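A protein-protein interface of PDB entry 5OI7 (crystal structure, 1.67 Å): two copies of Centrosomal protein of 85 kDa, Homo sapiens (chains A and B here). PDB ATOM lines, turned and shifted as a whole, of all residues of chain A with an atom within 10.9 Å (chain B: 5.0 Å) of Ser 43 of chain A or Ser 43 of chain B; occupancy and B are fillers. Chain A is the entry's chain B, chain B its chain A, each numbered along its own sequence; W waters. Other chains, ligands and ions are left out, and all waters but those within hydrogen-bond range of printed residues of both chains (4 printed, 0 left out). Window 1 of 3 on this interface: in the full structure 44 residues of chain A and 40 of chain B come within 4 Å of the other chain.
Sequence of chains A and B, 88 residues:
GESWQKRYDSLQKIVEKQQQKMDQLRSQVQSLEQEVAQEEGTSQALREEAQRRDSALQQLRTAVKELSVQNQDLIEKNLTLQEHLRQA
Of the 18 printed residues of chain A, 6 touch a printed residue of chain B. Hydrophobic or aromatic side chains of chain A that line the printed part of chain B: Leu 46. Hydrophobic or aromatic side chains of chain B within 4 Å of the printed part of chain A: Leu 46. Among the printed residues, 12 pairs touch across the chains. Among the printed residues, no Asp or Glu carboxylate lies within 4 Å of a Lys or Arg side-chain nitrogen of the other chain.
The side-chain carboxylate of Glu 39 of chain B is in hydrogen-bond range of the side-chain hydroxyl of Ser 43 of chain A, 2.7 Å away. The side-chain hydroxyl (OG) of Ser 43 of chain B is in hydrogen-bond range of the side-chain carboxylate (OE2) of Glu 39 of chain A (2.9 Å).
Of the printed residues of chain B, Ser 43 of chain A touches Glu 39, Ser 43 and Leu 46. Gly 41 of chain B touches none of the printed residues of chain A. No residue of chain A comes within 4 Å of Gln 44 of chain B. No residue of chain A comes within 4 Å of Ala 45 of chain B. Arg 47 of chain B touches just one residue of chain A: Thr 42 (3.6 Å). Of the printed residues of chain B, Glu 40 of chain A touches Glu 39 (3.7 Å). Of the printed residues of chain B, Thr 42 of chain A touches Ser 43 (3.7 Å) and Arg 47 (3.6 Å). Of the printed residues of chain B, Glu 39 of chain A touches Glu 39 (3.6 Å), Glu 40 (3.6 Å) and Ser 43 (2.9 Å). Gln 38 of chain A touches none of the printed residues of chain B. Ala 37 of chain A touches none of the printed residues of chain B. The nearest printed residue of chain A that does not touch Ser 43 of chain B is Glu 40 of chain A (5.9 Å). The nearest printed residue of chain B that does not touch Glu 39 of chain A is Arg 47 of chain B (4.7 Å).
Glu 39 of chain A touches Ser 43 of chain B, and with the chains exchanged Ser 43 of chain A touches Glu 39 of chain B. Ser 43 of chain B touches its own counterpart, Ser 43 of chain A. Leu 46 of chain A touches its own counterpart, Leu 46 of chain B. Arg 47 of chain A touches Leu 46 of chain B, but with the chains exchanged Leu 46 of chain A does not touch Arg 47 of chain B (4.1 Å). Of the 12 pairs that touch across the chains among the printed residues, 9 have their exchanged pair printed and touching as well.
Glu 39 of chain B touches Glu 39 of chain A (C to CG, 3.6 Å). Glu 39 of chain A touches Glu 40 of chain B (CG to N, 3.6 Å). Glu 40 of chain A touches Glu 39 of chain B (N to CG, 3.7 Å). OG of Ser 43 of chain B touches CG2 of Thr 42 of chain A, 3.7 Å away. CG2 of Thr 42 of chain A touches NH2 of Arg 47 of chain B, at 3.6 Å. N of Ser 43 of chain A touches OG of Ser 43 of chain B (3.5 Å). CD1 of Leu 46 of chain B touches O of Ser 43 of chain A, 3.5 Å away. Leu 46 of chain A touches Ser 43 of chain B (CD1 to O, 3.6 Å). Leu 46 of chain A touches Leu 46 of chain B (CB to CD1, 3.9 Å). Leu 46 of chain B touches Arg 47 of chain A.
Water W3 lies within hydrogen-bond range of the side-chain carboxylate of Glu 39 of chain B (2.5 Å), the guanidinium group of Arg 47 of chain A (3.0 Å) and the side-chain hydroxyl of Ser 43 of chain A (3.2 Å). Water W4 bridges the side-chain carboxylate of Glu 39 of chain B (2.6 Å) and the side-chain carboxylate of Glu 40 of chain A (3.1 Å). Water W2 bridges OE1 of Glu 39 of chain A (2.7 Å) and OE2 of Glu 40 of chain B (3.0 Å). Water W1 lies within hydrogen-bond range of the side-chain carboxylate of Glu 39 of chain A and the guanidinium group of Arg 47 of chain B.
O of Glu 39 of chain B sits at hydrogen-bond distance from OG of Ser 43 of chain B, at 3.5 Å. The backbone carbonyl oxygen of Gln 38 of chain A sits at hydrogen-bond distance from the side-chain hydroxyl of Thr 42 of chain A (3.3 Å). The backbone carbonyl oxygen of Glu 39 of chain A is in hydrogen-bond range of the side-chain hydroxyl of Ser 43 of chain A, 3.4 Å away. O of Glu 40 of chain A sits at hydrogen-bond distance from OG of Ser 43 of chain A (2.9 Å). OG of Ser 43 of chain A sits at hydrogen-bond distance from NH2 of Arg 47 of chain A (3.3 Å). The side-chain amide oxygen of Gln 44 of chain A lies within hydrogen-bond range of the guanidinium group of Arg 47 of chain A (3.0 Å).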
ATOM      1  N   GLU A  35      12.119  -3.218 -16.404  1.00  0.00           N
ATOM      2  CA  GLU A  35      11.953  -2.356 -15.236  1.00  0.00           C
ATOM      3  C   GLU A  35      10.769  -2.799 -14.390  1.00  0.00           C
ATOM      4  O   GLU A  35      10.848  -2.812 -13.155  1.00  0.00           O
ATOM      5  CB  GLU A  35      11.786  -0.897 -15.660  1.00  0.00           C
ATOM      6  CG  GLU A  35      13.059  -0.264 -16.189  1.00  0.00           C
ATOM      7  CD  GLU A  35      12.969   1.246 -16.280  1.00  0.00           C
ATOM      8  OE1 GLU A  35      11.915   1.806 -15.911  1.00  0.00           O
ATOM      9  OE2 GLU A  35      13.956   1.875 -16.720  1.00  0.00           O
ATOM     10  N   VAL A  36       9.656  -3.154 -15.037  1.00  0.00           N
ATOM     11  CA  VAL A  36       8.497  -3.652 -14.302  1.00  0.00           C
ATOM     12  C   VAL A  36       8.866  -4.903 -13.517  1.00  0.00           C
ATOM     13  O   VAL A  36       8.560  -5.024 -12.324  1.00  0.00           O
ATOM     14  CB  VAL A  36       7.325  -3.921 -15.261  1.00  0.00           C
ATOM     15  CG1 VAL A  36       6.206  -4.646 -14.524  1.00  0.00           C
ATOM     16  CG2 VAL A  36       6.818  -2.619 -15.858  1.00  0.00           C
ATOM     17  N   ALA A  37       9.524  -5.859 -14.178  1.00  0.00           N
ATOM     18  CA  ALA A  37       9.884  -7.103 -13.504  1.00  0.00           C
ATOM     19  C   ALA A  37      10.784  -6.838 -12.303  1.00  0.00           C
ATOM     20  O   ALA A  37      10.585  -7.414 -11.225  1.00  0.00           O
ATOM     21  CB  ALA A  37      10.567  -8.056 -14.485  1.00  0.00           C
ATOM     22  N   GLN A  38      11.781  -5.966 -12.467  1.00  0.00           N
ATOM     23  CA  GLN A  38      12.671  -5.653 -11.354  1.00  0.00           C
ATOM     24  C   GLN A  38      11.918  -4.978 -10.214  1.00  0.00           C
ATOM     25  O   GLN A  38      12.140  -5.297  -9.040  1.00  0.00           O
ATOM     26  CB  GLN A  38      13.821  -4.768 -11.837  1.00  0.00           C
ATOM     27  CG  GLN A  38      14.751  -5.465 -12.822  1.00  0.00           C
ATOM     28  CD  GLN A  38      15.753  -4.515 -13.457  1.00  0.00           C
ATOM     29  OE1 GLN A  38      15.657  -3.298 -13.301  1.00  0.00           O
ATOM     30  NE2 GLN A  38      16.720  -5.071 -14.179  1.00  0.00           N
ATOM     31  N   GLU A  39      11.021  -4.042 -10.537  1.00  0.00           N
ATOM     32  CA  GLU A  39      10.282  -3.343  -9.492  1.00  0.00           C
ATOM     33  C   GLU A  39       9.307  -4.274  -8.785  1.00  0.00           C
ATOM     34  O   GLU A  39       9.039  -4.097  -7.591  1.00  0.00           O
ATOM     35  CB  GLU A  39       9.536  -2.146 -10.080  1.00  0.00           C
ATOM     36  CG  GLU A  39       9.149  -1.110  -9.036  1.00  0.00           C
ATOM     37  CD  GLU A  39      10.358  -0.530  -8.326  1.00  0.00           C
ATOM     38  OE1 GLU A  39      11.433  -0.416  -8.960  1.00  0.00           O
ATOM     39  OE2 GLU A  39      10.237  -0.198  -7.129  1.00  0.00           O
ATOM     40  N   GLU A  40       8.767  -5.265  -9.500  1.00  0.00           N
ATOM     41  CA  GLU A  40       7.914  -6.258  -8.854  1.00  0.00           C
ATOM     42  C   GLU A  40       8.708  -7.093  -7.858  1.00  0.00           C
ATOM     43  O   GLU A  40       8.209  -7.432  -6.779  1.00  0.00           O
ATOM     44  CB  GLU A  40       7.256  -7.150  -9.908  1.00  0.00           C
ATOM     45  CG  GLU A  40       6.212  -6.416 -10.752  1.00  0.00           C
ATOM     46  CD  GLU A  40       5.638  -7.271 -11.866  1.00  0.00           C
ATOM     47  OE1 GLU A  40       6.399  -8.053 -12.474  1.00  0.00           O
ATOM     48  OE2 GLU A  40       4.421  -7.160 -12.129  1.00  0.00           O
ATOM     49  N   GLY A  41       9.952  -7.428  -8.196  1.00  0.00           N
ATOM     50  CA  GLY A  41      10.802  -8.098  -7.228  1.00  0.00           C
ATOM     51  C   GLY A  41      11.051  -7.251  -5.995  1.00  0.00           C
ATOM     52  O   GLY A  41      11.073  -7.761  -4.873  1.00  0.00           O
ATOM     53  N   THR A  42      11.252  -5.949  -6.187  1.00  0.00           N
ATOM     54  CA  THR A  42      11.456  -5.054  -5.054  1.00  0.00           C
ATOM     55  C   THR A  42      10.220  -5.011  -4.159  1.00  0.00           C
ATOM     56  O   THR A  42      10.323  -5.151  -2.933  1.00  0.00           O
ATOM     57  CB  THR A  42      11.812  -3.652  -5.556  1.00  0.00           C
ATOM     58  OG1 THR A  42      13.069  -3.690  -6.253  1.00  0.00           O
ATOM     59  CG2 THR A  42      11.898  -2.670  -4.393  1.00  0.00           C
ATOM     60  N   SER A  43       9.037  -4.827  -4.754  1.00  0.00           N
ATOM     61  CA  SER A  43       7.817  -4.755  -3.956  1.00  0.00           C
ATOM     62  C   SER A  43       7.562  -6.065  -3.221  1.00  0.00           C
ATOM     63  O   SER A  43       7.131  -6.059  -2.062  1.00  0.00           O
ATOM     64  CB  SER A  43       6.623  -4.393  -4.841  1.00  0.00           C
ATOM     65  OG  SER A  43       6.377  -5.390  -5.818  1.00  0.00           O
ATOM     66  N   GLN A  44       7.822  -7.201  -3.872  1.00  0.00           N
ATOM     67  CA  GLN A  44       7.607  -8.468  -3.179  1.00  0.00           C
ATOM     68  C   GLN A  44       8.581  -8.630  -2.019  1.00  0.00           C
ATOM     69  O   GLN A  44       8.203  -9.117  -0.949  1.00  0.00           O
ATOM     70  CB  GLN A  44       7.720  -9.649  -4.143  1.00  0.00           C
ATOM     71  CG  GLN A  44       7.387 -10.987  -3.471  1.00  0.00           C
ATOM     72  CD  GLN A  44       6.109 -10.925  -2.631  1.00  0.00           C
ATOM     73  OE1 GLN A  44       5.097 -10.368  -3.059  1.00  0.00           O
ATOM     74  NE2 GLN A  44       6.161 -11.490  -1.424  1.00  0.00           N
ATOM     75  N   ALA A  45       9.841  -8.225  -2.209  1.00  0.00           N
ATOM     76  CA  ALA A  45      10.799  -8.302  -1.110  1.00  0.00           C
ATOM     77  C   ALA A  45      10.377  -7.408   0.049  1.00  0.00           C
ATOM     78  O   ALA A  45      10.533  -7.776   1.218  1.00  0.00           O
ATOM     79  CB  ALA A  45      12.198  -7.922  -1.598  1.00  0.00           C
ATOM     80  N   LEU A  46       9.843  -6.222  -0.254  1.00  0.00           N
ATOM     81  CA  LEU A  46       9.376  -5.335   0.808  1.00  0.00           C
ATOM     82  C   LEU A  46       8.195  -5.940   1.559  1.00  0.00           C
ATOM     83  O   LEU A  46       8.104  -5.807   2.784  1.00  0.00           O
ATOM     84  CB  LEU A  46       9.006  -3.972   0.227  1.00  0.00           C
ATOM     85  CG  LEU A  46      10.182  -3.084  -0.183  1.00  0.00           C
ATOM     86  CD1 LEU A  46       9.740  -2.039  -1.200  1.00  0.00           C
ATOM     87  CD2 LEU A  46      10.808  -2.412   1.040  1.00  0.00           C
ATOM     88  N   ARG A  47       7.277  -6.596   0.845  1.00  0.00           N
ATOM     89  CA  ARG A  47       6.142  -7.229   1.514  1.00  0.00           C
ATOM     90  C   ARG A  47       6.608  -8.348   2.436  1.00  0.00           C
ATOM     91  O   ARG A  47       6.075  -8.519   3.539  1.00  0.00           O
ATOM     92  CB  ARG A  47       5.143  -7.766   0.486  1.00  0.00           C
ATOM     93  CG  ARG A  47       4.183  -6.718  -0.062  1.00  0.00           C
ATOM     94  CD  ARG A  47       3.131  -7.348  -0.978  1.00  0.00           C
ATOM     95  NE  ARG A  47       3.709  -7.817  -2.236  1.00  0.00           N
ATOM     96  CZ  ARG A  47       3.738  -7.105  -3.357  1.00  0.00           C
ATOM     97  NH1 ARG A  47       3.213  -5.889  -3.385  1.00  0.00           N
ATOM     98  NH2 ARG A  47       4.287  -7.614  -4.453  1.00  0.00           N
ATOM     99  N   GLU A  48       7.607  -9.119   2.007  1.00  0.00           N
ATOM    100  CA  GLU A  48       8.087 -10.213   2.846  1.00  0.00           C
ATOM    101  C   GLU A  48       8.807  -9.691   4.085  1.00  0.00           C
ATOM    102  O   GLU A  48       8.646 -10.242   5.178  1.00  0.00           O
ATOM    103  CB  GLU A  48       8.997 -11.138   2.042  1.00  0.00           C
ATOM    104  CG  GLU A  48       8.239 -12.052   1.095  1.00  0.00           C
ATOM    105  CD  GLU A  48       9.151 -12.999   0.342  1.00  0.00           C
ATOM    106  OE1 GLU A  48      10.366 -13.011   0.627  1.00  0.00           O
ATOM    107  OE2 GLU A  48       8.652 -13.734  -0.537  1.00  0.00           O
ATOM    108  N   GLU A  49       9.606  -8.634   3.938  1.00  0.00           N
ATOM    109  CA  GLU A  49      10.246  -8.050   5.112  1.00  0.00           C
ATOM    110  C   GLU A  49       9.215  -7.453   6.060  1.00  0.00           C
ATOM    111  O   GLU A  49       9.388  -7.514   7.285  1.00  0.00           O
ATOM    112  CB  GLU A  49      11.264  -6.993   4.683  1.00  0.00           C
ATOM    113  CG  GLU A  49      12.121  -6.452   5.823  1.00  0.00           C
ATOM    114  CD  GLU A  49      13.041  -7.503   6.428  1.00  0.00           C
ATOM    115  OE1 GLU A  49      13.337  -8.508   5.749  1.00  0.00           O
ATOM    116  OE2 GLU A  49      13.466  -7.324   7.590  1.00  0.00           O
ATOM    117  N   ALA A  50       8.136  -6.879   5.519  1.00  0.00           N
ATOM    118  CA  ALA A  50       7.082  -6.343   6.375  1.00  0.00           C
ATOM    119  C   ALA A  50       6.431  -7.446   7.204  1.00  0.00           C
ATOM    120  O   ALA A  50       6.079  -7.229   8.370  1.00  0.00           O
ATOM    121  CB  ALA A  50       6.034  -5.617   5.529  1.00  0.00           C
ATOM    122  N   GLN A  51       6.252  -8.633   6.617  1.00  0.00           N
ATOM    123  CA  GLN A  51       5.679  -9.750   7.364  1.00  0.00           C
ATOM    124  C   GLN A  51       6.576 -10.149   8.529  1.00  0.00           C
ATOM    125  O   GLN A  51       6.103 -10.354   9.653  1.00  0.00           O
ATOM    126  CB  GLN A  51       5.448 -10.945   6.441  1.00  0.00           C
ATOM    127  CG  GLN A  51       4.264 -10.804   5.507  1.00  0.00           C
ATOM    128  CD  GLN A  51       3.974 -12.090   4.755  1.00  0.00           C
ATOM    129  OE1 GLN A  51       4.608 -13.117   4.996  1.00  0.00           O
ATOM    130  NE2 GLN A  51       3.014 -12.038   3.841  1.00  0.00           N
ATOM    131  N   ARG A  52       7.881 -10.270   8.277  1.00  0.00           N
ATOM    132  CA  ARG A  52       8.801 -10.629   9.351  1.00  0.00           C
ATOM    133  C   ARG A  52       8.800  -9.579  10.452  1.00  0.00           C
ATOM    134  O   ARG A  52       8.827  -9.915  11.644  1.00  0.00           O
ATOM    135  CB  ARG A  52      10.212 -10.815   8.800  1.00  0.00           C
ATOM    136  CG  ARG A  52      10.420 -12.139   8.091  1.00  0.00           C
ATOM    137  CD  ARG A  52      11.878 -12.339   7.728  1.00  0.00           C
ATOM    138  NE  ARG A  52      12.285 -11.502   6.606  1.00  0.00           N
ATOM    139  CZ  ARG A  52      12.196 -11.875   5.335  1.00  0.00           C
ATOM    140  NH1 ARG A  52      11.716 -13.073   5.030  1.00  0.00           N
ATOM    141  NH2 ARG A  52      12.588 -11.055   4.369  1.00  0.00           N
ATOM    142  N   GLU B  39       4.085   0.436 -10.098  1.00  0.00           N
ATOM    143  CA  GLU B  39       4.884  -0.479  -9.287  1.00  0.00           C
ATOM    144  C   GLU B  39       5.895   0.280  -8.437  1.00  0.00           C
ATOM    145  O   GLU B  39       6.167  -0.106  -7.291  1.00  0.00           O
ATOM    146  CB  GLU B  39       5.583  -1.503 -10.182  1.00  0.00           C
ATOM    147  CG  GLU B  39       5.987  -2.769  -9.443  1.00  0.00           C
ATOM    148  CD  GLU B  39       4.804  -3.475  -8.811  1.00  0.00           C
ATOM    149  OE1 GLU B  39       3.700  -3.446  -9.403  1.00  0.00           O
ATOM    150  OE2 GLU B  39       4.978  -4.049  -7.717  1.00  0.00           O
ATOM    151  N   GLU B  40       6.471   1.358  -8.979  1.00  0.00           N
ATOM    152  CA  GLU B  40       7.332   2.211  -8.167  1.00  0.00           C
ATOM    153  C   GLU B  40       6.532   2.920  -7.085  1.00  0.00           C
ATOM    154  O   GLU B  40       7.034   3.119  -5.973  1.00  0.00           O
ATOM    155  CB  GLU B  40       8.063   3.221  -9.053  1.00  0.00           C
ATOM    156  CG  GLU B  40       9.016   2.571 -10.044  1.00  0.00           C
ATOM    157  CD  GLU B  40       9.825   3.576 -10.840  1.00  0.00           C
ATOM    158  OE1 GLU B  40       9.267   4.624 -11.227  1.00  0.00           O
ATOM    159  OE2 GLU B  40      11.023   3.314 -11.078  1.00  0.00           O
ATOM    160  N   GLY B  41       5.288   3.295  -7.381  1.00  0.00           N
ATOM    161  CA  GLY B  41       4.440   3.862  -6.345  1.00  0.00           C
ATOM    162  C   GLY B  41       4.126   2.858  -5.255  1.00  0.00           C
ATOM    163  O   GLY B  41       4.089   3.202  -4.070  1.00  0.00           O
ATOM    164  N   THR B  42       3.896   1.602  -5.638  1.00  0.00           N
ATOM    165  CA  THR B  42       3.676   0.555  -4.645  1.00  0.00           C
ATOM    166  C   THR B  42       4.907   0.366  -3.767  1.00  0.00           C
ATOM    167  O   THR B  42       4.799   0.289  -2.537  1.00  0.00           O
ATOM    168  CB  THR B  42       3.294  -0.749  -5.347  1.00  0.00           C
ATOM    169  OG1 THR B  42       2.023  -0.584  -5.987  1.00  0.00           O
ATOM    170  CG2 THR B  42       3.211  -1.904  -4.350  1.00  0.00           C
ATOM    171  N   SER B  43       6.094   0.295  -4.378  1.00  0.00           N
ATOM    172  CA  SER B  43       7.317   0.109  -3.599  1.00  0.00           C
ATOM    173  C   SER B  43       7.534   1.264  -2.627  1.00  0.00           C
ATOM    174  O   SER B  43       7.876   1.052  -1.458  1.00  0.00           O
ATOM    175  CB  SER B  43       8.520  -0.043  -4.531  1.00  0.00           C
ATOM    176  OG  SER B  43       8.559  -1.339  -5.102  1.00  0.00           O
ATOM    177  N   GLN B  44       7.344   2.502  -3.095  1.00  0.00           N
ATOM    178  CA  GLN B  44       7.551   3.651  -2.214  1.00  0.00           C
ATOM    179  C   GLN B  44       6.538   3.659  -1.072  1.00  0.00           C
ATOM    180  O   GLN B  44       6.870   4.029   0.060  1.00  0.00           O
ATOM    181  CB  GLN B  44       7.474   4.954  -3.009  1.00  0.00           C
ATOM    182  CG  GLN B  44       7.652   6.212  -2.163  1.00  0.00           C
ATOM    183  CD  GLN B  44       8.955   6.222  -1.369  1.00  0.00           C
ATOM    184  OE1 GLN B  44       9.964   5.663  -1.801  1.00  0.00           O
ATOM    185  NE2 GLN B  44       8.931   6.854  -0.197  1.00  0.00           N
ATOM    186  N   ALA B  45       5.292   3.267  -1.352  1.00  0.00           N
ATOM    187  CA  ALA B  45       4.298   3.189  -0.284  1.00  0.00           C
ATOM    188  C   ALA B  45       4.698   2.150   0.756  1.00  0.00           C
ATOM    189  O   ALA B  45       4.528   2.365   1.962  1.00  0.00           O
ATOM    190  CB  ALA B  45       2.922   2.867  -0.863  1.00  0.00           C
ATOM    191  N   LEU B  46       5.234   1.015   0.305  1.00  0.00           N
ATOM    192  CA  LEU B  46       5.704  -0.001   1.242  1.00  0.00           C
ATOM    193  C   LEU B  46       6.878   0.512   2.069  1.00  0.00           C
ATOM    194  O   LEU B  46       6.996   0.189   3.257  1.00  0.00           O
ATOM    195  CB  LEU B  46       6.081  -1.278   0.484  1.00  0.00           C
ATOM    196  CG  LEU B  46       4.936  -2.104  -0.115  1.00  0.00           C
ATOM    197  CD1 LEU B  46       5.450  -3.103  -1.156  1.00  0.00           C
ATOM    198  CD2 LEU B  46       4.166  -2.836   0.972  1.00  0.00           C
ATOM    199  N   ARG B  47       7.760   1.314   1.464  1.00  0.00           N
ATOM    200  CA  ARG B  47       8.852   1.910   2.233  1.00  0.00           C
ATOM    201  C   ARG B  47       8.321   2.887   3.276  1.00  0.00           C
ATOM    202  O   ARG B  47       8.862   2.975   4.383  1.00  0.00           O
ATOM    203  CB  ARG B  47       9.841   2.614   1.306  1.00  0.00           C
ATOM    204  CG  ARG B  47      10.682   1.665   0.473  1.00  0.00           C
ATOM    205  CD  ARG B  47      11.748   2.428  -0.301  1.00  0.00           C
ATOM    206  NE  ARG B  47      12.635   1.519  -1.012  1.00  0.00           N
ATOM    207  CZ  ARG B  47      12.458   1.136  -2.272  1.00  0.00           C
ATOM    208  NH1 ARG B  47      11.426   1.591  -2.971  1.00  0.00           N
ATOM    209  NH2 ARG B  47      13.319   0.295  -2.829  1.00  0.00           N
HETATM  210  O   HOH W   1      12.038   1.512  -6.046  1.00  0.00           O
HETATM  211  O   HOH W   2      12.942   1.763  -9.378  1.00  0.00           O
HETATM  212  O   HOH W   3       3.223  -5.290  -6.356  1.00  0.00           O
HETATM  213  O   HOH W   4       2.687  -5.777  -9.959  1.00  0.00           O
